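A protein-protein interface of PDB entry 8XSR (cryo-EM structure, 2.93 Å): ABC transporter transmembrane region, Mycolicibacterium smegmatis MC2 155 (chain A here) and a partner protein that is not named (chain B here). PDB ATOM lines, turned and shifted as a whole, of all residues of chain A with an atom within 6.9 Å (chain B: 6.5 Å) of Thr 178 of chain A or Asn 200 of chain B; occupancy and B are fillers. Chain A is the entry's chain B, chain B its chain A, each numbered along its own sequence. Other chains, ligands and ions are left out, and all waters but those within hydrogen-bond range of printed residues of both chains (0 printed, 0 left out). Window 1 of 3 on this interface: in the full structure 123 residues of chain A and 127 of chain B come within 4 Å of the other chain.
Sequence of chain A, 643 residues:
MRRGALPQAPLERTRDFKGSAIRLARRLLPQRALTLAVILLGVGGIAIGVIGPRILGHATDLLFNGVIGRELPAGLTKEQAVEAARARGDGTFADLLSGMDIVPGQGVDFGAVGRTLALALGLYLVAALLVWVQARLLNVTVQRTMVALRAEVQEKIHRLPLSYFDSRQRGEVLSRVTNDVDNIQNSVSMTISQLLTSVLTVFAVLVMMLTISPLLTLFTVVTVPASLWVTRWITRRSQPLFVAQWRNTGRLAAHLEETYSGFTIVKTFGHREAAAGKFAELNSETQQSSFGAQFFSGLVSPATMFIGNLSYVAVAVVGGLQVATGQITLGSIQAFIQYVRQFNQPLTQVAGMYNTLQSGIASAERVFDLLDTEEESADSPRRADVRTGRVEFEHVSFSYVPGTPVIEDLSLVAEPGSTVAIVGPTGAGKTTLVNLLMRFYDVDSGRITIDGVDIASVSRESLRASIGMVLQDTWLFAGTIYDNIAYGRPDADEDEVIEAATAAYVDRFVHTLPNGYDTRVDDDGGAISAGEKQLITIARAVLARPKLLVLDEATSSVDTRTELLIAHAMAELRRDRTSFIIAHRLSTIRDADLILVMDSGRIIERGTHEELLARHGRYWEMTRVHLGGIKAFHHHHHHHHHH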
ATOM      1  N   ARG A 150      -5.504  24.827  -1.105  1.00  0.00           N
ATOM      2  CA  ARG A 150      -5.020  25.330  -2.375  1.00  0.00           C
ATOM      3  C   ARG A 150      -3.506  25.243  -2.501  1.00  0.00           C
ATOM      4  O   ARG A 150      -2.983  25.404  -3.606  1.00  0.00           O
ATOM      5  CB  ARG A 150      -5.484  26.780  -2.530  1.00  0.00           C
ATOM      6  CG  ARG A 150      -5.364  27.361  -3.911  1.00  0.00           C
ATOM      7  CD  ARG A 150      -5.712  28.833  -3.893  1.00  0.00           C
ATOM      8  NE  ARG A 150      -7.106  29.113  -3.575  1.00  0.00           N
ATOM      9  CZ  ARG A 150      -8.076  29.176  -4.479  1.00  0.00           C
ATOM     10  NH1 ARG A 150      -7.806  28.974  -5.761  1.00  0.00           N
ATOM     11  NH2 ARG A 150      -9.315  29.445  -4.101  1.00  0.00           N
ATOM     12  N   VAL A 153      -2.791  21.280  -3.314  1.00  0.00           N
ATOM     13  CA  VAL A 153      -3.119  21.027  -4.708  1.00  0.00           C
ATOM     14  C   VAL A 153      -1.949  21.416  -5.597  1.00  0.00           C
ATOM     15  O   VAL A 153      -1.611  20.709  -6.551  1.00  0.00           O
ATOM     16  CB  VAL A 153      -4.402  21.780  -5.099  1.00  0.00           C
ATOM     17  CG1 VAL A 153      -4.683  21.613  -6.568  1.00  0.00           C
ATOM     18  CG2 VAL A 153      -5.576  21.279  -4.289  1.00  0.00           C
ATOM     19  N   VAL A 173      -8.832  19.237 -15.565  1.00  0.00           N
ATOM     20  CA  VAL A 173      -7.960  19.452 -14.416  1.00  0.00           C
ATOM     21  C   VAL A 173      -7.875  20.933 -14.077  1.00  0.00           C
ATOM     22  O   VAL A 173      -7.638  21.298 -12.921  1.00  0.00           O
ATOM     23  CB  VAL A 173      -6.571  18.843 -14.678  1.00  0.00           C
ATOM     24  CG1 VAL A 173      -5.653  19.064 -13.493  1.00  0.00           C
ATOM     25  CG2 VAL A 173      -6.694  17.364 -14.970  1.00  0.00           C
ATOM     26  N   LEU A 174      -8.095  21.808 -15.055  1.00  0.00           N
ATOM     27  CA  LEU A 174      -8.092  23.238 -14.779  1.00  0.00           C
ATOM     28  C   LEU A 174      -9.263  23.613 -13.886  1.00  0.00           C
ATOM     29  O   LEU A 174      -9.060  24.088 -12.767  1.00  0.00           O
ATOM     30  CB  LEU A 174      -8.129  24.052 -16.070  1.00  0.00           C
ATOM     31  CG  LEU A 174      -8.138  25.562 -15.832  1.00  0.00           C
ATOM     32  CD1 LEU A 174      -6.904  25.989 -15.070  1.00  0.00           C
ATOM     33  CD2 LEU A 174      -8.241  26.307 -17.147  1.00  0.00           C
ATOM     34  N   SER A 175     -10.492  23.382 -14.345  1.00  0.00           N
ATOM     35  CA  SER A 175     -11.645  23.710 -13.519  1.00  0.00           C
ATOM     36  C   SER A 175     -11.905  22.598 -12.513  1.00  0.00           C
ATOM     37  O   SER A 175     -13.035  22.121 -12.379  1.00  0.00           O
ATOM     38  CB  SER A 175     -12.882  23.940 -14.386  1.00  0.00           C
ATOM     39  OG  SER A 175     -13.282  22.739 -15.021  1.00  0.00           O
ATOM     40  N   ARG A 176     -10.855  22.181 -11.813  1.00  0.00           N
ATOM     41  CA  ARG A 176     -10.959  21.306 -10.656  1.00  0.00           C
ATOM     42  C   ARG A 176     -10.017  21.828  -9.584  1.00  0.00           C
ATOM     43  O   ARG A 176     -10.196  21.559  -8.393  1.00  0.00           O
ATOM     44  CB  ARG A 176     -10.636  19.858 -11.030  1.00  0.00           C
ATOM     45  CG  ARG A 176     -10.760  18.891  -9.875  1.00  0.00           C
ATOM     46  CD  ARG A 176     -10.577  17.454 -10.308  1.00  0.00           C
ATOM     47  NE  ARG A 176     -11.692  16.987 -11.125  1.00  0.00           N
ATOM     48  CZ  ARG A 176     -11.746  15.788 -11.694  1.00  0.00           C
ATOM     49  NH1 ARG A 176     -10.752  14.928 -11.525  1.00  0.00           N
ATOM     50  NH2 ARG A 176     -12.799  15.444 -12.422  1.00  0.00           N
ATOM     51  N   VAL A 177      -9.007  22.583 -10.011  1.00  0.00           N
ATOM     52  CA  VAL A 177      -8.079  23.241  -9.104  1.00  0.00           C
ATOM     53  C   VAL A 177      -8.422  24.711  -8.922  1.00  0.00           C
ATOM     54  O   VAL A 177      -7.893  25.360  -8.017  1.00  0.00           O
ATOM     55  CB  VAL A 177      -6.629  23.088  -9.590  1.00  0.00           C
ATOM     56  CG1 VAL A 177      -6.273  21.630  -9.749  1.00  0.00           C
ATOM     57  CG2 VAL A 177      -6.435  23.827 -10.888  1.00  0.00           C
ATOM     58  N   THR A 178      -9.300  25.255  -9.763  1.00  0.00           N
ATOM     59  CA  THR A 178      -9.609  26.679  -9.706  1.00  0.00           C
ATOM     60  C   THR A 178     -11.084  26.995  -9.505  1.00  0.00           C
ATOM     61  O   THR A 178     -11.386  28.018  -8.885  1.00  0.00           O
ATOM     62  CB  THR A 178      -9.114  27.389 -10.977  1.00  0.00           C
ATOM     63  OG1 THR A 178      -9.194  28.805 -10.793  1.00  0.00           O
ATOM     64  CG2 THR A 178      -9.951  27.013 -12.182  1.00  0.00           C
ATOM     65  N   ASN A 179     -12.015  26.170  -9.987  1.00  0.00           N
ATOM     66  CA  ASN A 179     -13.430  26.372  -9.727  1.00  0.00           C
ATOM     67  C   ASN A 179     -13.985  25.459  -8.654  1.00  0.00           C
ATOM     68  O   ASN A 179     -14.951  25.840  -7.989  1.00  0.00           O
ATOM     69  CB  ASN A 179     -14.257  26.174 -11.007  1.00  0.00           C
ATOM     70  CG  ASN A 179     -14.080  27.304 -11.994  1.00  0.00           C
ATOM     71  OD1 ASN A 179     -14.021  28.472 -11.612  1.00  0.00           O
ATOM     72  ND2 ASN A 179     -14.008  26.965 -13.274  1.00  0.00           N
ATOM     73  N   ASP A 180     -13.413  24.275  -8.465  1.00  0.00           N
ATOM     74  CA  ASP A 180     -13.842  23.404  -7.387  1.00  0.00           C
ATOM     75  C   ASP A 180     -13.209  23.769  -6.055  1.00  0.00           C
ATOM     76  O   ASP A 180     -13.639  23.248  -5.023  1.00  0.00           O
ATOM     77  CB  ASP A 180     -13.520  21.945  -7.713  1.00  0.00           C
ATOM     78  CG  ASP A 180     -14.290  21.437  -8.911  1.00  0.00           C
ATOM     79  OD1 ASP A 180     -15.352  22.009  -9.231  1.00  0.00           O
ATOM     80  OD2 ASP A 180     -13.843  20.450  -9.525  1.00  0.00           O
ATOM     81  N   VAL A 181     -12.201  24.639  -6.051  1.00  0.00           N
ATOM     82  CA  VAL A 181     -11.583  25.083  -4.809  1.00  0.00           C
ATOM     83  C   VAL A 181     -12.249  26.389  -4.395  1.00  0.00           C
ATOM     84  O   VAL A 181     -12.164  26.811  -3.237  1.00  0.00           O
ATOM     85  CB  VAL A 181     -10.058  25.231  -4.968  1.00  0.00           C
ATOM     86  CG1 VAL A 181      -9.417  25.693  -3.676  1.00  0.00           C
ATOM     87  CG2 VAL A 181      -9.453  23.916  -5.399  1.00  0.00           C
ATOM     88  N   ASP A 182     -12.950  27.025  -5.335  1.00  0.00           N
ATOM     89  CA  ASP A 182     -13.808  28.155  -5.017  1.00  0.00           C
ATOM     90  C   ASP A 182     -15.186  27.744  -4.529  1.00  0.00           C
ATOM     91  O   ASP A 182     -15.850  28.547  -3.869  1.00  0.00           O
ATOM     92  CB  ASP A 182     -13.972  29.074  -6.237  1.00  0.00           C
ATOM     93  CG  ASP A 182     -12.741  29.916  -6.506  1.00  0.00           C
ATOM     94  OD1 ASP A 182     -12.025  30.246  -5.539  1.00  0.00           O
ATOM     95  OD2 ASP A 182     -12.493  30.255  -7.681  1.00  0.00           O
ATOM     96  N   ASN A 183     -15.629  26.527  -4.835  1.00  0.00           N
ATOM     97  CA  ASN A 183     -16.886  26.024  -4.305  1.00  0.00           C
ATOM     98  C   ASN A 183     -16.723  25.359  -2.951  1.00  0.00           C
ATOM     99  O   ASN A 183     -17.685  25.315  -2.179  1.00  0.00           O
ATOM    100  CB  ASN A 183     -17.523  25.029  -5.276  1.00  0.00           C
ATOM    101  CG  ASN A 183     -18.030  25.689  -6.533  1.00  0.00           C
ATOM    102  OD1 ASN A 183     -18.559  26.799  -6.496  1.00  0.00           O
ATOM    103  ND2 ASN A 183     -17.894  25.001  -7.656  1.00  0.00           N
ATOM    104  N   LEU B 195      -7.222  39.759  -7.713  1.00  0.00           N
ATOM    105  CA  LEU B 195      -6.236  38.920  -7.063  1.00  0.00           C
ATOM    106  C   LEU B 195      -6.706  37.476  -6.975  1.00  0.00           C
ATOM    107  O   LEU B 195      -5.876  36.569  -6.873  1.00  0.00           O
ATOM    108  CB  LEU B 195      -5.926  39.498  -5.680  1.00  0.00           C
ATOM    109  CG  LEU B 195      -4.711  39.055  -4.888  1.00  0.00           C
ATOM    110  CD1 LEU B 195      -3.468  39.336  -5.685  1.00  0.00           C
ATOM    111  CD2 LEU B 195      -4.686  39.864  -3.631  1.00  0.00           C
ATOM    112  N   ILE B 196      -8.018  37.249  -7.014  1.00  0.00           N
ATOM    113  CA  ILE B 196      -8.576  35.958  -7.387  1.00  0.00           C
ATOM    114  C   ILE B 196      -8.346  35.649  -8.857  1.00  0.00           C
ATOM    115  O   ILE B 196      -8.062  34.490  -9.193  1.00  0.00           O
ATOM    116  CB  ILE B 196     -10.085  35.888  -7.068  1.00  0.00           C
ATOM    117  CG1 ILE B 196     -10.339  36.031  -5.573  1.00  0.00           C
ATOM    118  CG2 ILE B 196     -10.688  34.590  -7.562  1.00  0.00           C
ATOM    119  CD1 ILE B 196     -11.778  36.288  -5.230  1.00  0.00           C
ATOM    120  N   ASP B 197      -8.447  36.640  -9.736  1.00  0.00           N
ATOM    121  CA  ASP B 197      -8.223  36.473 -11.163  1.00  0.00           C
ATOM    122  C   ASP B 197      -6.756  36.236 -11.499  1.00  0.00           C
ATOM    123  O   ASP B 197      -6.451  35.798 -12.610  1.00  0.00           O
ATOM    124  CB  ASP B 197      -8.740  37.715 -11.902  1.00  0.00           C
ATOM    125  CG  ASP B 197      -8.944  37.485 -13.388  1.00  0.00           C
ATOM    126  OD1 ASP B 197      -8.715  36.357 -13.873  1.00  0.00           O
ATOM    127  OD2 ASP B 197      -9.339  38.447 -14.080  1.00  0.00           O
ATOM    128  N   GLY B 198      -5.847  36.493 -10.563  1.00  0.00           N
ATOM    129  CA  GLY B 198      -4.431  36.309 -10.811  1.00  0.00           C
ATOM    130  C   GLY B 198      -3.940  34.943 -10.390  1.00  0.00           C
ATOM    131  O   GLY B 198      -3.083  34.350 -11.050  1.00  0.00           O
ATOM    132  N   ILE B 199      -4.470  34.453  -9.273  1.00  0.00           N
ATOM    133  CA  ILE B 199      -4.101  33.141  -8.764  1.00  0.00           C
ATOM    134  C   ILE B 199      -4.600  32.096  -9.749  1.00  0.00           C
ATOM    135  O   ILE B 199      -3.973  31.054  -9.942  1.00  0.00           O
ATOM    136  CB  ILE B 199      -4.714  32.876  -7.378  1.00  0.00           C
ATOM    137  CG1 ILE B 199      -4.687  31.380  -7.061  1.00  0.00           C
ATOM    138  CG2 ILE B 199      -6.135  33.415  -7.313  1.00  0.00           C
ATOM    139  CD1 ILE B 199      -4.060  31.051  -5.723  1.00  0.00           C
ATOM    140  N   ASN B 200      -5.738  32.388 -10.370  1.00  0.00           N
ATOM    141  CA  ASN B 200      -6.322  31.496 -11.359  1.00  0.00           C
ATOM    142  C   ASN B 200      -5.462  31.510 -12.614  1.00  0.00           C
ATOM    143  O   ASN B 200      -5.277  30.484 -13.267  1.00  0.00           O
ATOM    144  CB  ASN B 200      -7.753  31.921 -11.688  1.00  0.00           C
ATOM    145  CG  ASN B 200      -8.640  31.976 -10.459  1.00  0.00           C
ATOM    146  OD1 ASN B 200      -8.467  31.200  -9.519  1.00  0.00           O
ATOM    147  ND2 ASN B 200      -9.597  32.896 -10.460  1.00  0.00           N
ATOM    148  N   ARG B 201      -4.938  32.687 -12.943  1.00  0.00           N
ATOM    149  CA  ARG B 201      -4.074  32.839 -14.103  1.00  0.00           C
ATOM    150  C   ARG B 201      -2.839  31.977 -13.885  1.00  0.00           C
ATOM    151  O   ARG B 201      -2.396  31.264 -14.786  1.00  0.00           O
ATOM    152  CB  ARG B 201      -3.674  34.303 -14.289  1.00  0.00           C
ATOM    153  CG  ARG B 201      -2.881  34.576 -15.556  1.00  0.00           C
ATOM    154  CD  ARG B 201      -2.794  36.066 -15.844  1.00  0.00           C
ATOM    155  NE  ARG B 201      -4.111  36.659 -16.056  1.00  0.00           N
ATOM    156  CZ  ARG B 201      -4.366  37.961 -15.977  1.00  0.00           C
ATOM    157  NH1 ARG B 201      -5.595  38.413 -16.185  1.00  0.00           N
ATOM    158  NH2 ARG B 201      -3.392  38.813 -15.688  1.00  0.00           N
ATOM    159  N   VAL B 202      -2.289  32.051 -12.678  1.00  0.00           N
ATOM    160  CA  VAL B 202      -1.117  31.257 -12.315  1.00  0.00           C
ATOM    161  C   VAL B 202      -1.408  29.770 -12.479  1.00  0.00           C
ATOM    162  O   VAL B 202      -0.604  29.022 -13.043  1.00  0.00           O
ATOM    163  CB  VAL B 202      -0.665  31.588 -10.882  1.00  0.00           C
ATOM    164  CG1 VAL B 202       0.404  30.625 -10.430  1.00  0.00           C
ATOM    165  CG2 VAL B 202      -0.150  33.005 -10.812  1.00  0.00           C
ATOM    166  N   LEU B 203      -2.568  29.321 -11.993  1.00  0.00           N
ATOM    167  CA  LEU B 203      -2.917  27.908 -12.119  1.00  0.00           C
ATOM    168  C   LEU B 203      -3.110  27.504 -13.575  1.00  0.00           C
ATOM    169  O   LEU B 203      -2.697  26.412 -13.983  1.00  0.00           O
ATOM    170  CB  LEU B 203      -4.172  27.603 -11.308  1.00  0.00           C
ATOM    171  CG  LEU B 203      -3.977  27.649  -9.797  1.00  0.00           C
ATOM    172  CD1 LEU B 203      -5.308  27.542  -9.092  1.00  0.00           C
ATOM    173  CD2 LEU B 203      -3.056  26.520  -9.382  1.00  0.00           C
ATOM    174  N   ARG B 204      -3.739  28.367 -14.372  1.00  0.00           N
ATOM    175  CA  ARG B 204      -3.933  28.073 -15.786  1.00  0.00           C
ATOM    176  C   ARG B 204      -2.605  27.970 -16.521  1.00  0.00           C
ATOM    177  O   ARG B 204      -2.412  27.066 -17.341  1.00  0.00           O
ATOM    178  CB  ARG B 204      -4.811  29.148 -16.416  1.00  0.00           C
ATOM    179  CG  ARG B 204      -5.143  28.913 -17.866  1.00  0.00           C
ATOM    180  CD  ARG B 204      -5.985  30.046 -18.399  1.00  0.00           C
ATOM    181  NE  ARG B 204      -5.237  31.297 -18.418  1.00  0.00           N
ATOM    182  CZ  ARG B 204      -5.775  32.488 -18.659  1.00  0.00           C
ATOM    183  NH1 ARG B 204      -5.014  33.575 -18.655  1.00  0.00           N
ATOM    184  NH2 ARG B 204      -7.073  32.593 -18.904  1.00  0.00           N
ATOM    185  N   ASP B 205      -1.673  28.881 -16.238  1.00  0.00           N
ATOM    186  CA  ASP B 205      -0.362  28.826 -16.867  1.00  0.00           C
ATOM    187  C   ASP B 205       0.470  27.654 -16.373  1.00  0.00           C
ATOM    188  O   ASP B 205       1.320  27.162 -17.119  1.00  0.00           O
ATOM    189  CB  ASP B 205       0.394  30.130 -16.627  1.00  0.00           C
ATOM    190  CG  ASP B 205      -0.164  31.280 -17.433  1.00  0.00           C
ATOM    191  OD1 ASP B 205      -0.684  31.033 -18.540  1.00  0.00           O
ATOM    192  OD2 ASP B 205      -0.083  32.432 -16.962  1.00  0.00           O
ATOM    193  N   PHE B 226       3.452  30.697  -6.905  1.00  0.00           N
ATOM    194  CA  PHE B 226       2.096  30.433  -6.448  1.00  0.00           C
ATOM    195  C   PHE B 226       1.906  30.675  -4.961  1.00  0.00           C
ATOM    196  O   PHE B 226       0.807  31.043  -4.544  1.00  0.00           O
ATOM    197  CB  PHE B 226       1.703  28.989  -6.754  1.00  0.00           C
ATOM    198  CG  PHE B 226       0.325  28.630  -6.296  1.00  0.00           C
ATOM    199  CD1 PHE B 226      -0.783  28.997  -7.031  1.00  0.00           C
ATOM    200  CD2 PHE B 226       0.136  27.936  -5.118  1.00  0.00           C
ATOM    201  CE1 PHE B 226      -2.048  28.667  -6.605  1.00  0.00           C
ATOM    202  CE2 PHE B 226      -1.123  27.610  -4.691  1.00  0.00           C
ATOM    203  CZ  PHE B 226      -2.217  27.972  -5.434  1.00  0.00           C
ATOM    204  N   LEU B 233      -3.599  36.677  -1.907  1.00  0.00           N
ATOM    205  CA  LEU B 233      -5.047  36.546  -1.984  1.00  0.00           C
ATOM    206  C   LEU B 233      -5.663  36.372  -0.608  1.00  0.00           C
ATOM    207  O   LEU B 233      -6.687  36.987  -0.303  1.00  0.00           O
ATOM    208  CB  LEU B 233      -5.415  35.370  -2.882  1.00  0.00           C
ATOM    209  CG  LEU B 233      -6.909  35.072  -2.932  1.00  0.00           C
ATOM    210  CD1 LEU B 233      -7.664  36.298  -3.381  1.00  0.00           C
ATOM    211  CD2 LEU B 233      -7.169  33.908  -3.860  1.00  0.00           C
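Ile 199 of chain B touches Arg 150 of chain A (CD1 to CD, 3.3 Å). Arg 150 of chain A touches Phe 226 of chain B. Leu 174 of chain A touches Arg 204 of chain B (CD1 to CA, 3.7 Å). Val 177 of chain A touches Leu 203 of chain B (O to CD1, 3.5 Å).
OD1 of Asn 200 of chain B sits at hydrogen-bond distance from OG1 of Thr 178 of chain A, at 2.8 Å.
Hydrophobic or aromatic side chains of chain A that line the printed part of chain B: Leu 174. Of the 13 printed residues of chain B, 5 touch a printed residue of chain A. Among the printed residues, 5 pairs touch across the chains. Among the printed residues, no Asp or Glu carboxylate lies within 4 Å of a Lys or Arg side-chain nitrogen of the other chain.
Of chain A, only Thr 178 (2.8 Å) comes within 4 Å of Asn 200 of chain B. Printed residues of chain A within 4 Å of Ile 199 of chain B: Arg 150. Of the printed residues of chain B, Arg 150 of chain A touches Ile 199 (3.3 Å) and Phe 226 (3.1 Å). Printed residues of chain A within 4 Å of Arg 204 of chain B: Leu 174 (3.7 Å). Of the printed residues of chain A, Phe 226 of chain B touches Arg 150 (3.1 Å). The nearest residue of chain A that does not touch Asn 200 of chain B is Arg 150 of chain A (4.4 Å).
NH2 of Arg 150 of chain A is in salt-bridge range of OD1 of Asp 182 of chain A (3.2 Å). The backbone carbonyl oxygen (O) of Ile 196 of chain B sits at hydrogen-bond distance from the side-chain amide nitrogen (ND2) of Asn 200 of chain B, 2.5 Å away.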
